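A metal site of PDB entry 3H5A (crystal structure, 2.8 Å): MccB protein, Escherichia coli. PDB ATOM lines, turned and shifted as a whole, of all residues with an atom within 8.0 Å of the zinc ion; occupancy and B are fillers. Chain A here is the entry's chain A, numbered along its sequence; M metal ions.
The backbone NH of Val 345 sits close to the side-chain sulfur of Cys 343.
The guanidinium group of Arg 339 sits at hydrogen-bond distance from the backbone carbonyl oxygen of Cys 346 (3.3 Å).
The side-chain sulfur (SG) of Cys 260 lies close to the backbone NH (N) of Ser 340 (3.2 Å).
The side-chain amide oxygen of Asn 224 sits close to the side-chain sulfur of Cys 257 (3.2 Å).
SG of Cys 257 lies close to N of Glu 259.
The side-chain hydroxyl (OG) of Ser 340 is in hydrogen-bond range of the backbone NH (N) of Cys 343 (3.2 Å).
The zinc ion is bound by SG of Cys 346 (2.4 Å), SG of Cys 343 (2.5 Å), SG of Cys 257 (2.5 Å) and SG of Cys 260 (2.6 Å).
Four residues have an atom within 4 Å of the zinc ion: Cys 257, Cys 260, Cys 343 and Cys 346.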
ATOM      1  N   ASN A 224      19.763  -8.992  -1.080  1.00  0.00           N
ATOM      2  CA  ASN A 224      20.969  -8.619  -1.833  1.00  0.00           C
ATOM      3  C   ASN A 224      22.212  -9.242  -1.257  1.00  0.00           C
ATOM      4  O   ASN A 224      23.001  -9.801  -2.012  1.00  0.00           O
ATOM      5  CB  ASN A 224      21.168  -7.125  -1.907  1.00  0.00           C
ATOM      6  CG  ASN A 224      22.372  -6.731  -2.743  1.00  0.00           C
ATOM      7  OD1 ASN A 224      23.365  -6.205  -2.231  1.00  0.00           O
ATOM      8  ND2 ASN A 224      22.291  -6.991  -4.043  1.00  0.00           N
ATOM      9  N   VAL A 228      24.256 -12.233  -3.146  1.00  0.00           N
ATOM     10  CA  VAL A 228      25.674 -12.029  -3.441  1.00  0.00           C
ATOM     11  C   VAL A 228      26.487 -13.222  -2.883  1.00  0.00           C
ATOM     12  O   VAL A 228      27.302 -13.822  -3.596  1.00  0.00           O
ATOM     13  CB  VAL A 228      26.196 -10.710  -2.846  1.00  0.00           C
ATOM     14  CG1 VAL A 228      27.707 -10.690  -2.818  1.00  0.00           C
ATOM     15  CG2 VAL A 228      25.662  -9.548  -3.647  1.00  0.00           C
ATOM     16  N   TYR A 250      20.191  -8.629 -10.541  1.00  0.00           N
ATOM     17  CA  TYR A 250      21.556  -9.001 -10.139  1.00  0.00           C
ATOM     18  C   TYR A 250      22.029 -10.339 -10.741  1.00  0.00           C
ATOM     19  O   TYR A 250      21.407 -11.369 -10.493  1.00  0.00           O
ATOM     20  CB  TYR A 250      21.667  -9.069  -8.616  1.00  0.00           C
ATOM     21  CG  TYR A 250      22.961  -9.687  -8.158  1.00  0.00           C
ATOM     22  CD1 TYR A 250      24.159  -8.963  -8.229  1.00  0.00           C
ATOM     23  CD2 TYR A 250      23.008 -11.011  -7.646  1.00  0.00           C
ATOM     24  CE1 TYR A 250      25.379  -9.529  -7.809  1.00  0.00           C
ATOM     25  CE2 TYR A 250      24.228 -11.577  -7.226  1.00  0.00           C
ATOM     26  CZ  TYR A 250      25.400 -10.828  -7.306  1.00  0.00           C
ATOM     27  OH  TYR A 250      26.606 -11.345  -6.930  1.00  0.00           O
ATOM     28  N   THR A 255      27.554  -8.242 -12.972  1.00  0.00           N
ATOM     29  CA  THR A 255      26.645  -7.129 -12.739  1.00  0.00           C
ATOM     30  C   THR A 255      26.876  -6.460 -11.380  1.00  0.00           C
ATOM     31  O   THR A 255      27.556  -7.006 -10.512  1.00  0.00           O
ATOM     32  CB  THR A 255      25.179  -7.636 -12.862  1.00  0.00           C
ATOM     33  OG1 THR A 255      24.451  -6.820 -13.784  1.00  0.00           O
ATOM     34  CG2 THR A 255      24.449  -7.651 -11.526  1.00  0.00           C
ATOM     35  N   GLY A 256      26.297  -5.271 -11.206  1.00  0.00           N
ATOM     36  CA  GLY A 256      26.304  -4.614  -9.910  1.00  0.00           C
ATOM     37  C   GLY A 256      25.245  -5.172  -8.993  1.00  0.00           C
ATOM     38  O   GLY A 256      24.309  -5.845  -9.425  1.00  0.00           O
ATOM     39  N   CYS A 257      25.389  -4.906  -7.702  1.00  0.00           N
ATOM     40  CA  CYS A 257      24.419  -5.372  -6.724  1.00  0.00           C
ATOM     41  C   CYS A 257      23.683  -4.180  -6.166  1.00  0.00           C
ATOM     42  O   CYS A 257      23.982  -3.041  -6.497  1.00  0.00           O
ATOM     43  CB  CYS A 257      25.096  -6.215  -5.620  1.00  0.00           C
ATOM     44  SG  CYS A 257      25.772  -5.359  -4.153  1.00  0.00           S
ATOM     45  N   TYR A 258      22.711  -4.424  -5.303  1.00  0.00           N
ATOM     46  CA  TYR A 258      21.916  -3.339  -4.787  1.00  0.00           C
ATOM     47  C   TYR A 258      22.757  -2.264  -4.043  1.00  0.00           C
ATOM     48  O   TYR A 258      22.331  -1.121  -3.892  1.00  0.00           O
ATOM     49  CB  TYR A 258      20.805  -3.889  -3.895  1.00  0.00           C
ATOM     50  CG  TYR A 258      19.712  -2.907  -3.555  1.00  0.00           C
ATOM     51  CD1 TYR A 258      18.718  -2.582  -4.483  1.00  0.00           C
ATOM     52  CD2 TYR A 258      19.657  -2.324  -2.294  1.00  0.00           C
ATOM     53  CE1 TYR A 258      17.712  -1.704  -4.162  1.00  0.00           C
ATOM     54  CE2 TYR A 258      18.656  -1.427  -1.966  1.00  0.00           C
ATOM     55  CZ  TYR A 258      17.684  -1.138  -2.903  1.00  0.00           C
ATOM     56  OH  TYR A 258      16.683  -0.248  -2.564  1.00  0.00           O
ATOM     57  N   GLU A 259      23.953  -2.618  -3.622  1.00  0.00           N
ATOM     58  CA  GLU A 259      24.726  -1.694  -2.802  1.00  0.00           C
ATOM     59  C   GLU A 259      25.922  -1.109  -3.526  1.00  0.00           C
ATOM     60  O   GLU A 259      26.600  -0.255  -2.992  1.00  0.00           O
ATOM     61  CB  GLU A 259      25.148  -2.376  -1.513  1.00  0.00           C
ATOM     62  CG  GLU A 259      24.825  -1.545  -0.298  1.00  0.00           C
ATOM     63  CD  GLU A 259      23.984  -2.349   0.671  1.00  0.00           C
ATOM     64  OE1 GLU A 259      24.539  -2.836   1.700  1.00  0.00           O
ATOM     65  OE2 GLU A 259      22.774  -2.521   0.380  1.00  0.00           O
ATOM     66  N   CYS A 260      26.169  -1.543  -4.755  1.00  0.00           N
ATOM     67  CA  CYS A 260      27.262  -1.018  -5.552  1.00  0.00           C
ATOM     68  C   CYS A 260      27.338   0.525  -5.617  1.00  0.00           C
ATOM     69  O   CYS A 260      28.396   1.077  -5.885  1.00  0.00           O
ATOM     70  CB  CYS A 260      27.240  -1.612  -6.944  1.00  0.00           C
ATOM     71  SG  CYS A 260      28.168  -3.158  -7.142  1.00  0.00           S
ATOM     72  N   GLN A 261      26.235   1.228  -5.367  1.00  0.00           N
ATOM     73  CA  GLN A 261      26.243   2.697  -5.324  1.00  0.00           C
ATOM     74  C   GLN A 261      25.333   3.190  -4.173  1.00  0.00           C
ATOM     75  O   GLN A 261      25.116   2.460  -3.197  1.00  0.00           O
ATOM     76  CB  GLN A 261      25.827   3.296  -6.676  1.00  0.00           C
ATOM     77  CG  GLN A 261      26.343   2.555  -7.914  1.00  0.00           C
ATOM     78  CD  GLN A 261      27.744   2.946  -8.298  1.00  0.00           C
ATOM     79  OE1 GLN A 261      28.237   3.990  -7.882  1.00  0.00           O
ATOM     80  NE2 GLN A 261      28.405   2.111  -9.088  1.00  0.00           N
ATOM     81  N   MET A 337      23.295   1.441 -10.941  1.00  0.00           N
ATOM     82  CA  MET A 337      23.757   0.473  -9.960  1.00  0.00           C
ATOM     83  C   MET A 337      24.756  -0.477 -10.606  1.00  0.00           C
ATOM     84  O   MET A 337      24.729  -1.689 -10.381  1.00  0.00           O
ATOM     85  CB  MET A 337      22.570  -0.260  -9.322  1.00  0.00           C
ATOM     86  CG  MET A 337      21.618   0.658  -8.537  1.00  0.00           C
ATOM     87  SD  MET A 337      20.470  -0.204  -7.413  1.00  0.00           S
ATOM     88  CE  MET A 337      20.635  -1.816  -8.100  1.00  0.00           C
ATOM     89  N   GLY A 338      25.642   0.099 -11.434  1.00  0.00           N
ATOM     90  CA  GLY A 338      26.671  -0.649 -12.136  1.00  0.00           C
ATOM     91  C   GLY A 338      27.741  -1.075 -11.145  1.00  0.00           C
ATOM     92  O   GLY A 338      27.892  -0.500 -10.071  1.00  0.00           O
ATOM     93  N   ARG A 339      28.491  -2.101 -11.520  1.00  0.00           N
ATOM     94  CA  ARG A 339      29.374  -2.783 -10.580  1.00  0.00           C
ATOM     95  C   ARG A 339      30.447  -1.835 -10.022  1.00  0.00           C
ATOM     96  O   ARG A 339      31.048  -1.086 -10.784  1.00  0.00           O
ATOM     97  CB  ARG A 339      29.986  -4.033 -11.228  1.00  0.00           C
ATOM     98  CG  ARG A 339      30.833  -4.830 -10.282  1.00  0.00           C
ATOM     99  CD  ARG A 339      30.826  -6.315 -10.597  1.00  0.00           C
ATOM    100  NE  ARG A 339      31.370  -7.040  -9.439  1.00  0.00           N
ATOM    101  CZ  ARG A 339      32.160  -8.114  -9.500  1.00  0.00           C
ATOM    102  NH1 ARG A 339      32.595  -8.667  -8.388  1.00  0.00           N
ATOM    103  NH2 ARG A 339      32.519  -8.618 -10.684  1.00  0.00           N
ATOM    104  N   SER A 340      30.649  -1.867  -8.706  1.00  0.00           N
ATOM    105  CA  SER A 340      31.760  -1.159  -8.035  1.00  0.00           C
ATOM    106  C   SER A 340      32.815  -2.172  -7.516  1.00  0.00           C
ATOM    107  O   SER A 340      32.476  -3.081  -6.759  1.00  0.00           O
ATOM    108  CB  SER A 340      31.225  -0.290  -6.869  1.00  0.00           C
ATOM    109  OG  SER A 340      32.277   0.300  -6.098  1.00  0.00           O
ATOM    110  N   PRO A 341      34.105  -1.996  -7.914  1.00  0.00           N
ATOM    111  CA  PRO A 341      35.196  -2.844  -7.417  1.00  0.00           C
ATOM    112  C   PRO A 341      35.346  -2.735  -5.897  1.00  0.00           C
ATOM    113  O   PRO A 341      35.878  -3.625  -5.227  1.00  0.00           O
ATOM    114  CB  PRO A 341      36.434  -2.264  -8.116  1.00  0.00           C
ATOM    115  CG  PRO A 341      35.896  -1.572  -9.351  1.00  0.00           C
ATOM    116  CD  PRO A 341      34.606  -0.972  -8.865  1.00  0.00           C
ATOM    117  N   VAL A 342      34.791  -1.637  -5.371  1.00  0.00           N
ATOM    118  CA  VAL A 342      35.017  -1.174  -4.010  1.00  0.00           C
ATOM    119  C   VAL A 342      33.781  -1.376  -3.110  1.00  0.00           C
ATOM    120  O   VAL A 342      33.810  -1.126  -1.894  1.00  0.00           O
ATOM    121  CB  VAL A 342      35.491   0.305  -4.075  1.00  0.00           C
ATOM    122  CG1 VAL A 342      35.144   1.096  -2.802  1.00  0.00           C
ATOM    123  CG2 VAL A 342      36.984   0.345  -4.391  1.00  0.00           C
ATOM    124  N   CYS A 343      32.709  -1.847  -3.719  1.00  0.00           N
ATOM    125  CA  CYS A 343      31.490  -2.203  -3.017  1.00  0.00           C
ATOM    126  C   CYS A 343      31.736  -3.024  -1.742  1.00  0.00           C
ATOM    127  O   CYS A 343      32.501  -4.003  -1.749  1.00  0.00           O
ATOM    128  CB  CYS A 343      30.585  -2.988  -3.937  1.00  0.00           C
ATOM    129  SG  CYS A 343      29.155  -3.526  -3.078  1.00  0.00           S
ATOM    130  N   SER A 344      31.070  -2.644  -0.670  1.00  0.00           N
ATOM    131  CA  SER A 344      31.268  -3.352   0.599  1.00  0.00           C
ATOM    132  C   SER A 344      30.417  -4.625   0.748  1.00  0.00           C
ATOM    133  O   SER A 344      30.437  -5.252   1.796  1.00  0.00           O
ATOM    134  CB  SER A 344      31.049  -2.415   1.780  1.00  0.00           C
ATOM    135  OG  SER A 344      29.772  -1.825   1.678  1.00  0.00           O
ATOM    136  N   VAL A 345      29.685  -5.000  -0.298  1.00  0.00           N
ATOM    137  CA  VAL A 345      29.007  -6.301  -0.309  1.00  0.00           C
ATOM    138  C   VAL A 345      29.630  -7.302  -1.320  1.00  0.00           C
ATOM    139  O   VAL A 345      29.897  -8.456  -0.964  1.00  0.00           O
ATOM    140  CB  VAL A 345      27.471  -6.156  -0.453  1.00  0.00           C
ATOM    141  CG1 VAL A 345      26.777  -7.520  -0.587  1.00  0.00           C
ATOM    142  CG2 VAL A 345      26.921  -5.413   0.749  1.00  0.00           C
ATOM    143  N   CYS A 346      29.908  -6.875  -2.544  1.00  0.00           N
ATOM    144  CA  CYS A 346      30.393  -7.797  -3.567  1.00  0.00           C
ATOM    145  C   CYS A 346      31.791  -7.473  -4.145  1.00  0.00           C
ATOM    146  O   CYS A 346      32.234  -8.101  -5.124  1.00  0.00           O
ATOM    147  CB  CYS A 346      29.371  -7.916  -4.707  1.00  0.00           C
ATOM    148  SG  CYS A 346      29.333  -6.487  -5.799  1.00  0.00           S
ATOM    149  N   GLY A 347      32.457  -6.481  -3.533  1.00  0.00           N
ATOM    150  CA  GLY A 347      33.779  -6.050  -3.972  1.00  0.00           C
ATOM    151  C   GLY A 347      34.913  -6.557  -3.092  1.00  0.00           C
ATOM    152  O   GLY A 347      34.727  -6.790  -1.899  1.00  0.00           O
HETATM  153 ZN    ZN M   1      28.024  -4.597  -5.024  1.00  0.00          ZN
